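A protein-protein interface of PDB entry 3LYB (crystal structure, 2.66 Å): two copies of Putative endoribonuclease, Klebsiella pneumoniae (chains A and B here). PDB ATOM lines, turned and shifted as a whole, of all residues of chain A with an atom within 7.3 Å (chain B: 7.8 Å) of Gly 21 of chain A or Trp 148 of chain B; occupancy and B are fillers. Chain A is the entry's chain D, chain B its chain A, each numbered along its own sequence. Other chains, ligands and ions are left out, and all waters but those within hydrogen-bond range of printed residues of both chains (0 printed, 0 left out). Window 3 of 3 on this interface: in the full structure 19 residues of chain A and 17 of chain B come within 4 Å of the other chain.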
ATOM      1  N   ARG A  18     -26.329 -10.732   2.463  1.00  0.00           N
ATOM      2  CA  ARG A  18     -25.129 -10.199   1.831  1.00  0.00           C
ATOM      3  C   ARG A  18     -24.443  -9.195   2.724  1.00  0.00           C
ATOM      4  O   ARG A  18     -25.087  -8.417   3.426  1.00  0.00           O
ATOM      5  CB  ARG A  18     -25.378  -9.647   0.418  1.00  0.00           C
ATOM      6  CG  ARG A  18     -25.289 -10.743  -0.652  1.00  0.00           C
ATOM      7  CD  ARG A  18     -25.503 -10.256  -2.084  1.00  0.00           C
ATOM      8  NE  ARG A  18     -24.334  -9.549  -2.606  1.00  0.00           N
ATOM      9  CZ  ARG A  18     -24.291  -8.933  -3.783  1.00  0.00           C
ATOM     10  NH1 ARG A  18     -25.356  -8.926  -4.588  1.00  0.00           N
ATOM     11  NH2 ARG A  18     -23.181  -8.312  -4.158  1.00  0.00           N
ATOM     12  N   ARG A  19     -23.118  -9.280   2.712  1.00  0.00           N
ATOM     13  CA  ARG A  19     -22.243  -8.476   3.534  1.00  0.00           C
ATOM     14  C   ARG A  19     -21.818  -7.257   2.747  1.00  0.00           C
ATOM     15  O   ARG A  19     -21.385  -7.378   1.600  1.00  0.00           O
ATOM     16  CB  ARG A  19     -21.029  -9.322   3.912  1.00  0.00           C
ATOM     17  CG  ARG A  19     -19.753  -8.535   4.235  1.00  0.00           C
ATOM     18  CD  ARG A  19     -19.094  -9.072   5.489  1.00  0.00           C
ATOM     19  NE  ARG A  19     -19.130  -8.055   6.524  1.00  0.00           N
ATOM     20  CZ  ARG A  19     -19.295  -8.287   7.826  1.00  0.00           C
ATOM     21  NH1 ARG A  19     -19.481  -9.517   8.291  1.00  0.00           N
ATOM     22  NH2 ARG A  19     -19.298  -7.261   8.663  1.00  0.00           N
ATOM     23  N   ALA A  20     -21.952  -6.086   3.353  1.00  0.00           N
ATOM     24  CA  ALA A  20     -21.501  -4.840   2.724  1.00  0.00           C
ATOM     25  C   ALA A  20     -20.845  -3.944   3.764  1.00  0.00           C
ATOM     26  O   ALA A  20     -21.539  -3.254   4.523  1.00  0.00           O
ATOM     27  CB  ALA A  20     -22.663  -4.118   2.071  1.00  0.00           C
ATOM     28  N   GLY A  21     -19.515  -3.965   3.804  1.00  0.00           N
ATOM     29  CA  GLY A  21     -18.769  -3.266   4.847  1.00  0.00           C
ATOM     30  C   GLY A  21     -18.980  -3.918   6.198  1.00  0.00           C
ATOM     31  O   GLY A  21     -18.808  -5.127   6.347  1.00  0.00           O
ATOM     32  N   ASP A  22     -19.383  -3.116   7.176  1.00  0.00           N
ATOM     33  CA  ASP A  22     -19.718  -3.624   8.519  1.00  0.00           C
ATOM     34  C   ASP A  22     -21.180  -4.097   8.651  1.00  0.00           C
ATOM     35  O   ASP A  22     -21.570  -4.620   9.717  1.00  0.00           O
ATOM     36  CB  ASP A  22     -19.403  -2.567   9.597  1.00  0.00           C
ATOM     37  CG  ASP A  22     -17.961  -2.047   9.512  1.00  0.00           C
ATOM     38  OD1 ASP A  22     -17.002  -2.867   9.415  1.00  0.00           O
ATOM     39  OD2 ASP A  22     -17.791  -0.810   9.523  1.00  0.00           O
ATOM     40  N   PHE A  23     -21.982  -3.918   7.591  1.00  0.00           N
ATOM     41  CA  PHE A  23     -23.405  -4.273   7.662  1.00  0.00           C
ATOM     42  C   PHE A  23     -23.732  -5.596   7.000  1.00  0.00           C
ATOM     43  O   PHE A  23     -23.125  -5.981   6.002  1.00  0.00           O
ATOM     44  CB  PHE A  23     -24.303  -3.199   7.038  1.00  0.00           C
ATOM     45  CG  PHE A  23     -24.300  -1.878   7.760  1.00  0.00           C
ATOM     46  CD1 PHE A  23     -23.380  -0.888   7.426  1.00  0.00           C
ATOM     47  CD2 PHE A  23     -25.247  -1.604   8.732  1.00  0.00           C
ATOM     48  CE1 PHE A  23     -23.381   0.347   8.076  1.00  0.00           C
ATOM     49  CE2 PHE A  23     -25.264  -0.362   9.382  1.00  0.00           C
ATOM     50  CZ  PHE A  23     -24.328   0.613   9.047  1.00  0.00           C
ATOM     51  N   ILE A  24     -24.722  -6.284   7.546  1.00  0.00           N
ATOM     52  CA  ILE A  24     -25.275  -7.436   6.860  1.00  0.00           C
ATOM     53  C   ILE A  24     -26.752  -7.199   6.578  1.00  0.00           C
ATOM     54  O   ILE A  24     -27.542  -6.951   7.504  1.00  0.00           O
ATOM     55  CB  ILE A  24     -24.998  -8.755   7.617  1.00  0.00           C
ATOM     56  CG1 ILE A  24     -23.482  -9.063   7.535  1.00  0.00           C
ATOM     57  CG2 ILE A  24     -25.847  -9.896   7.048  1.00  0.00           C
ATOM     58  CD1 ILE A  24     -23.033 -10.442   8.038  1.00  0.00           C
ATOM     59  N   PHE A  25     -27.098  -7.250   5.287  1.00  0.00           N
ATOM     60  CA  PHE A  25     -28.483  -7.198   4.812  1.00  0.00           C
ATOM     61  C   PHE A  25     -29.040  -8.587   4.601  1.00  0.00           C
ATOM     62  O   PHE A  25     -28.453  -9.414   3.924  1.00  0.00           O
ATOM     63  CB  PHE A  25     -28.572  -6.426   3.500  1.00  0.00           C
ATOM     64  CG  PHE A  25     -28.184  -5.001   3.625  1.00  0.00           C
ATOM     65  CD1 PHE A  25     -26.914  -4.577   3.209  1.00  0.00           C
ATOM     66  CD2 PHE A  25     -29.066  -4.078   4.190  1.00  0.00           C
ATOM     67  CE1 PHE A  25     -26.516  -3.226   3.336  1.00  0.00           C
ATOM     68  CE2 PHE A  25     -28.701  -2.718   4.323  1.00  0.00           C
ATOM     69  CZ  PHE A  25     -27.416  -2.285   3.894  1.00  0.00           C
ATOM     70  N   LEU A 149     -22.586  -5.781  12.075  1.00  0.00           N
ATOM     71  CA  LEU A 149     -21.601  -6.756  12.575  1.00  0.00           C
ATOM     72  C   LEU A 149     -20.226  -6.662  11.870  1.00  0.00           C
ATOM     73  O   LEU A 149     -19.938  -7.461  10.978  1.00  0.00           O
ATOM     74  CB  LEU A 149     -22.185  -8.166  12.420  1.00  0.00           C
ATOM     75  CG  LEU A 149     -21.431  -9.436  12.812  1.00  0.00           C
ATOM     76  CD1 LEU A 149     -21.454  -9.666  14.309  1.00  0.00           C
ATOM     77  CD2 LEU A 149     -22.057 -10.603  12.115  1.00  0.00           C
ATOM     78  N   PRO A 150     -19.371  -5.698  12.276  1.00  0.00           N
ATOM     79  CA  PRO A 150     -17.974  -5.634  11.756  1.00  0.00           C
ATOM     80  C   PRO A 150     -17.137  -6.888  12.073  1.00  0.00           C
ATOM     81  O   PRO A 150     -16.765  -7.642  11.161  1.00  0.00           O
ATOM     82  CB  PRO A 150     -17.369  -4.424  12.489  1.00  0.00           C
ATOM     83  CG  PRO A 150     -18.554  -3.634  13.018  1.00  0.00           C
ATOM     84  CD  PRO A 150     -19.648  -4.643  13.273  1.00  0.00           C
ATOM     85  N   ARG B  19     -24.642   9.598  -2.326  1.00  0.00           N
ATOM     86  CA  ARG B  19     -23.562   8.838  -1.675  1.00  0.00           C
ATOM     87  C   ARG B  19     -23.463   9.209  -0.200  1.00  0.00           C
ATOM     88  O   ARG B  19     -23.439  10.385   0.143  1.00  0.00           O
ATOM     89  CB  ARG B  19     -22.204   9.062  -2.347  1.00  0.00           C
ATOM     90  CG  ARG B  19     -21.030   8.451  -1.537  1.00  0.00           C
ATOM     91  CD  ARG B  19     -19.659   8.567  -2.221  1.00  0.00           C
ATOM     92  NE  ARG B  19     -19.544   7.741  -3.425  1.00  0.00           N
ATOM     93  CZ  ARG B  19     -19.314   6.431  -3.425  1.00  0.00           C
ATOM     94  NH1 ARG B  19     -19.174   5.756  -2.288  1.00  0.00           N
ATOM     95  NH2 ARG B  19     -19.240   5.790  -4.575  1.00  0.00           N
ATOM     96  N   ALA B  20     -23.425   8.202   0.661  1.00  0.00           N
ATOM     97  CA  ALA B  20     -23.092   8.392   2.053  1.00  0.00           C
ATOM     98  C   ALA B  20     -22.041   7.352   2.342  1.00  0.00           C
ATOM     99  O   ALA B  20     -22.327   6.151   2.314  1.00  0.00           O
ATOM    100  CB  ALA B  20     -24.297   8.170   2.918  1.00  0.00           C
ATOM    101  N   GLY B  21     -20.816   7.803   2.582  1.00  0.00           N
ATOM    102  CA  GLY B  21     -19.697   6.898   2.825  1.00  0.00           C
ATOM    103  C   GLY B  21     -19.449   6.000   1.634  1.00  0.00           C
ATOM    104  O   GLY B  21     -19.225   6.477   0.517  1.00  0.00           O
ATOM    105  N   ASP B  22     -19.516   4.693   1.883  1.00  0.00           N
ATOM    106  CA  ASP B  22     -19.311   3.674   0.856  1.00  0.00           C
ATOM    107  C   ASP B  22     -20.607   3.342   0.113  1.00  0.00           C
ATOM    108  O   ASP B  22     -20.582   2.839  -1.018  1.00  0.00           O
ATOM    109  CB  ASP B  22     -18.737   2.408   1.501  1.00  0.00           C
ATOM    110  CG  ASP B  22     -17.309   2.606   2.028  1.00  0.00           C
ATOM    111  OD1 ASP B  22     -16.538   3.438   1.468  1.00  0.00           O
ATOM    112  OD2 ASP B  22     -16.958   1.912   3.009  1.00  0.00           O
ATOM    113  N   PHE B  23     -21.743   3.608   0.754  1.00  0.00           N
ATOM    114  CA  PHE B  23     -23.023   3.308   0.133  1.00  0.00           C
ATOM    115  C   PHE B  23     -23.511   4.448  -0.737  1.00  0.00           C
ATOM    116  O   PHE B  23     -23.270   5.623  -0.448  1.00  0.00           O
ATOM    117  CB  PHE B  23     -24.082   3.003   1.169  1.00  0.00           C
ATOM    118  CG  PHE B  23     -23.811   1.782   1.987  1.00  0.00           C
ATOM    119  CD1 PHE B  23     -24.264   0.551   1.580  1.00  0.00           C
ATOM    120  CD2 PHE B  23     -23.146   1.880   3.196  1.00  0.00           C
ATOM    121  CE1 PHE B  23     -24.052  -0.578   2.355  1.00  0.00           C
ATOM    122  CE2 PHE B  23     -22.910   0.767   3.969  1.00  0.00           C
ATOM    123  CZ  PHE B  23     -23.372  -0.473   3.554  1.00  0.00           C
ATOM    124  N   ILE B  24     -24.180   4.082  -1.823  1.00  0.00           N
ATOM    125  CA  ILE B  24     -25.002   5.021  -2.573  1.00  0.00           C
ATOM    126  C   ILE B  24     -26.470   4.597  -2.472  1.00  0.00           C
ATOM    127  O   ILE B  24     -26.813   3.405  -2.581  1.00  0.00           O
ATOM    128  CB  ILE B  24     -24.569   5.132  -4.047  1.00  0.00           C
ATOM    129  CG1 ILE B  24     -23.160   5.750  -4.153  1.00  0.00           C
ATOM    130  CG2 ILE B  24     -25.574   5.995  -4.820  1.00  0.00           C
ATOM    131  CD1 ILE B  24     -22.524   5.591  -5.520  1.00  0.00           C
ATOM    132  N   PHE B  25     -27.328   5.577  -2.225  1.00  0.00           N
ATOM    133  CA  PHE B  25     -28.761   5.306  -2.064  1.00  0.00           C
ATOM    134  C   PHE B  25     -29.522   5.881  -3.221  1.00  0.00           C
ATOM    135  O   PHE B  25     -29.325   7.040  -3.585  1.00  0.00           O
ATOM    136  CB  PHE B  25     -29.307   5.869  -0.742  1.00  0.00           C
ATOM    137  CG  PHE B  25     -28.771   5.169   0.489  1.00  0.00           C
ATOM    138  CD1 PHE B  25     -27.660   5.683   1.179  1.00  0.00           C
ATOM    139  CD2 PHE B  25     -29.368   3.997   0.963  1.00  0.00           C
ATOM    140  CE1 PHE B  25     -27.172   5.050   2.323  1.00  0.00           C
ATOM    141  CE2 PHE B  25     -28.877   3.352   2.116  1.00  0.00           C
ATOM    142  CZ  PHE B  25     -27.777   3.884   2.793  1.00  0.00           C
ATOM    143  N   VAL B  84     -26.210   3.356 -11.772  1.00  0.00           N
ATOM    144  CA  VAL B  84     -25.026   2.776 -11.144  1.00  0.00           C
ATOM    145  C   VAL B  84     -23.789   2.784 -12.058  1.00  0.00           C
ATOM    146  O   VAL B  84     -22.675   3.045 -11.576  1.00  0.00           O
ATOM    147  CB  VAL B  84     -25.327   1.366 -10.594  1.00  0.00           C
ATOM    148  CG1 VAL B  84     -24.090   0.656 -10.114  1.00  0.00           C
ATOM    149  CG2 VAL B  84     -26.292   1.477  -9.454  1.00  0.00           C
ATOM    150  N   GLY B  89     -19.963   2.104 -10.809  1.00  0.00           N
ATOM    151  CA  GLY B  89     -20.315   0.779 -10.268  1.00  0.00           C
ATOM    152  C   GLY B  89     -20.914  -0.226 -11.237  1.00  0.00           C
ATOM    153  O   GLY B  89     -20.979   0.006 -12.428  1.00  0.00           O
ATOM    154  N   GLN B  90     -21.375  -1.349 -10.709  1.00  0.00           N
ATOM    155  CA  GLN B  90     -21.969  -2.410 -11.520  1.00  0.00           C
ATOM    156  C   GLN B  90     -23.170  -3.057 -10.812  1.00  0.00           C
ATOM    157  O   GLN B  90     -23.400  -2.791  -9.625  1.00  0.00           O
ATOM    158  CB  GLN B  90     -20.929  -3.485 -11.777  1.00  0.00           C
ATOM    159  CG  GLN B  90     -20.013  -3.188 -12.899  1.00  0.00           C
ATOM    160  CD  GLN B  90     -19.060  -4.330 -13.120  1.00  0.00           C
ATOM    161  OE1 GLN B  90     -18.746  -5.086 -12.186  1.00  0.00           O
ATOM    162  NE2 GLN B  90     -18.598  -4.481 -14.356  1.00  0.00           N
ATOM    163  N   SER B  92     -23.410  -5.957  -9.690  1.00  0.00           N
ATOM    164  CA  SER B  92     -22.926  -6.708  -8.521  1.00  0.00           C
ATOM    165  C   SER B  92     -22.714  -5.829  -7.281  1.00  0.00           C
ATOM    166  O   SER B  92     -22.636  -6.330  -6.154  1.00  0.00           O
ATOM    167  CB  SER B  92     -21.661  -7.531  -8.850  1.00  0.00           C
ATOM    168  OG  SER B  92     -20.661  -6.736  -9.473  1.00  0.00           O
ATOM    169  N   ASP B  93     -22.637  -4.524  -7.500  1.00  0.00           N
ATOM    170  CA  ASP B  93     -22.505  -3.559  -6.424  1.00  0.00           C
ATOM    171  C   ASP B  93     -23.869  -3.185  -5.835  1.00  0.00           C
ATOM    172  O   ASP B  93     -23.969  -2.669  -4.706  1.00  0.00           O
ATOM    173  CB  ASP B  93     -21.763  -2.324  -6.947  1.00  0.00           C
ATOM    174  CG  ASP B  93     -20.376  -2.672  -7.496  1.00  0.00           C
ATOM    175  OD1 ASP B  93     -19.640  -3.402  -6.777  1.00  0.00           O
ATOM    176  OD2 ASP B  93     -20.021  -2.228  -8.628  1.00  0.00           O
ATOM    177  N   VAL B  94     -24.918  -3.433  -6.617  1.00  0.00           N
ATOM    178  CA  VAL B  94     -26.270  -3.194  -6.166  1.00  0.00           C
ATOM    179  C   VAL B  94     -26.639  -4.387  -5.301  1.00  0.00           C
ATOM    180  O   VAL B  94     -27.109  -5.400  -5.799  1.00  0.00           O
ATOM    181  CB  VAL B  94     -27.263  -3.036  -7.356  1.00  0.00           C
ATOM    182  CG1 VAL B  94     -28.652  -2.667  -6.854  1.00  0.00           C
ATOM    183  CG2 VAL B  94     -26.778  -1.975  -8.356  1.00  0.00           C
ATOM    184  N   ILE B  95     -26.416  -4.254  -4.004  1.00  0.00           N
ATOM    185  CA  ILE B  95     -26.527  -5.373  -3.085  1.00  0.00           C
ATOM    186  C   ILE B  95     -27.961  -5.725  -2.639  1.00  0.00           C
ATOM    187  O   ILE B  95     -28.254  -6.906  -2.376  1.00  0.00           O
ATOM    188  CB  ILE B  95     -25.625  -5.165  -1.850  1.00  0.00           C
ATOM    189  CG1 ILE B  95     -25.481  -3.684  -1.516  1.00  0.00           C
ATOM    190  CG2 ILE B  95     -24.235  -5.729  -2.123  1.00  0.00           C
ATOM    191  CD1 ILE B  95     -26.310  -3.248  -0.370  1.00  0.00           C
ATOM    192  N   LYS B  96     -28.837  -4.709  -2.591  1.00  0.00           N
ATOM    193  CA  LYS B  96     -30.178  -4.821  -2.005  1.00  0.00           C
ATOM    194  C   LYS B  96     -31.283  -4.193  -2.862  1.00  0.00           C
ATOM    195  O   LYS B  96     -31.169  -3.050  -3.357  1.00  0.00           O
ATOM    196  CB  LYS B  96     -30.181  -4.148  -0.640  1.00  0.00           C
ATOM    197  CG  LYS B  96     -31.537  -4.026   0.008  1.00  0.00           C
ATOM    198  CD  LYS B  96     -31.513  -3.028   1.149  1.00  0.00           C
ATOM    199  CE  LYS B  96     -32.749  -3.146   2.031  1.00  0.00           C
ATOM    200  NZ  LYS B  96     -32.586  -4.264   2.987  1.00  0.00           N
ATOM    201  N   ALA B 145     -33.270   0.608  -4.928  1.00  0.00           N
ATOM    202  CA  ALA B 145     -31.979  -0.041  -4.972  1.00  0.00           C
ATOM    203  C   ALA B 145     -30.991   0.563  -3.961  1.00  0.00           C
ATOM    204  O   ALA B 145     -30.952   1.780  -3.747  1.00  0.00           O
ATOM    205  CB  ALA B 145     -31.425   0.012  -6.381  1.00  0.00           C
ATOM    206  N   THR B 146     -30.213  -0.303  -3.325  1.00  0.00           N
ATOM    207  CA  THR B 146     -29.111   0.127  -2.465  1.00  0.00           C
ATOM    208  C   THR B 146     -27.747  -0.425  -2.969  1.00  0.00           C
ATOM    209  O   THR B 146     -27.588  -1.643  -3.184  1.00  0.00           O
ATOM    210  CB  THR B 146     -29.343  -0.251  -0.977  1.00  0.00           C
ATOM    211  OG1 THR B 146     -30.421   0.511  -0.449  1.00  0.00           O
ATOM    212  CG2 THR B 146     -28.131   0.091  -0.168  1.00  0.00           C
ATOM    213  N   VAL B 147     -26.788   0.491  -3.133  1.00  0.00           N
ATOM    214  CA  VAL B 147     -25.463   0.188  -3.713  1.00  0.00           C
ATOM    215  C   VAL B 147     -24.334   0.333  -2.682  1.00  0.00           C
ATOM    216  O   VAL B 147     -24.260   1.348  -1.979  1.00  0.00           O
ATOM    217  CB  VAL B 147     -25.138   1.127  -4.902  1.00  0.00           C
ATOM    218  CG1 VAL B 147     -23.895   0.659  -5.622  1.00  0.00           C
ATOM    219  CG2 VAL B 147     -26.298   1.201  -5.875  1.00  0.00           C
ATOM    220  N   TRP B 148     -23.477  -0.681  -2.589  1.00  0.00           N
ATOM    221  CA  TRP B 148     -22.201  -0.562  -1.863  1.00  0.00           C
ATOM    222  C   TRP B 148     -21.030  -0.437  -2.849  1.00  0.00           C
ATOM    223  O   TRP B 148     -20.665  -1.406  -3.524  1.00  0.00           O
ATOM    224  CB  TRP B 148     -21.986  -1.745  -0.913  1.00  0.00           C
ATOM    225  CG  TRP B 148     -20.733  -1.661  -0.059  1.00  0.00           C
ATOM    226  CD1 TRP B 148     -20.478  -0.776   0.970  1.00  0.00           C
ATOM    227  CD2 TRP B 148     -19.585  -2.520  -0.138  1.00  0.00           C
ATOM    228  NE1 TRP B 148     -19.241  -1.036   1.522  1.00  0.00           N
ATOM    229  CE2 TRP B 148     -18.672  -2.095   0.860  1.00  0.00           C
ATOM    230  CE3 TRP B 148     -19.237  -3.608  -0.958  1.00  0.00           C
ATOM    231  CZ2 TRP B 148     -17.433  -2.708   1.047  1.00  0.00           C
ATOM    232  CZ3 TRP B 148     -18.004  -4.227  -0.760  1.00  0.00           C
ATOM    233  CH2 TRP B 148     -17.119  -3.775   0.241  1.00  0.00           C
ATOM    234  N   LEU B 149     -20.467   0.768  -2.925  1.00  0.00           N
ATOM    235  CA  LEU B 149     -19.386   1.079  -3.863  1.00  0.00           C
ATOM    236  C   LEU B 149     -18.304   2.003  -3.251  1.00  0.00           C
ATOM    237  O   LEU B 149     -18.336   3.238  -3.446  1.00  0.00           O
ATOM    238  CB  LEU B 149     -19.970   1.709  -5.126  1.00  0.00           C
ATOM    239  CG  LEU B 149     -19.029   2.167  -6.253  1.00  0.00           C
ATOM    240  CD1 LEU B 149     -18.464   0.980  -7.064  1.00  0.00           C
ATOM    241  CD2 LEU B 149     -19.729   3.145  -7.179  1.00  0.00           C
ATOM    242  N   PRO B 150     -17.347   1.411  -2.496  1.00  0.00           N
ATOM    243  CA  PRO B 150     -16.134   2.141  -1.968  1.00  0.00           C
ATOM    244  C   PRO B 150     -15.237   2.773  -3.050  1.00  0.00           C
ATOM    245  O   PRO B 150     -15.306   3.989  -3.286  1.00  0.00           O
ATOM    246  CB  PRO B 150     -15.344   1.050  -1.225  1.00  0.00           C
ATOM    247  CG  PRO B 150     -16.024  -0.308  -1.618  1.00  0.00           C
ATOM    248  CD  PRO B 150     -17.444   0.019  -2.000  1.00  0.00           C
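The guanidinium group of Arg 18 of chain A is in hydrogen-bond range of the backbone carbonyl oxygen of Ser 92 of chain B, 2.9 Å away.
The backbone carbonyl oxygen (O) of Asp 93 of chain B lies within hydrogen-bond range of the backbone NH (N) of Trp 148 of chain B (2.9 Å).
N of Ile 95 of chain B lies within hydrogen-bond range of O of Thr 146 of chain B, at 3.0 Å.
O of Lys 96 of chain B sits at hydrogen-bond distance from N of Thr 146 of chain B (2.9 Å).
N of Arg 18 of chain A lies within hydrogen-bond range of O of Phe 25 of chain A (2.9 Å).
The backbone carbonyl oxygen (O) of Gly 21 of chain A is in hydrogen-bond range of the guanidinium group (NE) of Arg 19 of chain A, at 3.0 Å.
CG2 of Ile 95 of chain B touches NH2 of Arg 18 of chain A, 3.5 Å away.
Phe 23 of chain B touches Ala 20 of chain A.
Trp 148 of chain B touches Ala 20 of chain A (CG to CB, 3.8 Å).
Gly 21 of chain A touches Trp 148 of chain B (N to CE2, 3.6 Å).
CE2 of Phe 23 of chain B touches CD1 of Phe 23 of chain A, at 3.9 Å.
CE1 of Phe 23 of chain B touches CE1 of Phe 25 of chain A, 3.7 Å away.
CE1 of Phe 25 of chain A touches CD1 of Ile 95 of chain B, 3.7 Å away.
CD2 of Phe 25 of chain A touches NZ of Lys 96 of chain B (3.7 Å).
Of the printed residues of chain B, Arg 18 of chain A touches Ser 92 (2.9 Å) and Ile 95 (3.5 Å).
Gly 21 of chain A touches just one residue of chain B: Trp 148.
Printed residues of chain B within 4 Å of Phe 25 of chain A: Phe 23 (3.7 Å), Ile 95 (3.7 Å) and Lys 96 (3.7 Å).
Printed residues of chain A within 4 Å of Phe 23 of chain B: Ala 20, Phe 23 and Phe 25.
Printed residues of chain A within 4 Å of Ile 95 of chain B: Arg 18 and Phe 25.
Printed residues of chain A within 4 Å of Lys 96 of chain B: Phe 25.
Printed residues of chain B that touch a printed residue of chain A: Phe 23, Ser 92, Ile 95, Lys 96 and Trp 148.
Hydrophobic or aromatic side chains of chain B that line the printed part of chain A: Phe 23, Ile 95 and Trp 148.
Among the printed residues, 9 pairs touch across the chains.
Ala 20 of chain A touches Phe 23 of chain B, but with the chains exchanged Phe 23 of chain A does not touch Ala 20 of chain B (8.2 Å).
Phe 23 of chain A touches its own counterpart, Phe 23 of chain B.
Phe 25 of chain A touches Phe 23 of chain B, but with the chains exchanged Phe 23 of chain A does not touch Phe 25 of chain B (7.7 Å).
Positions printed for both chains: 19, 20, 21, 22, 23, 24, 25, 149 and 150.
Of the 9 pairs that touch across the chains among the printed residues, 1 has its exchanged pair printed and touching as well.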
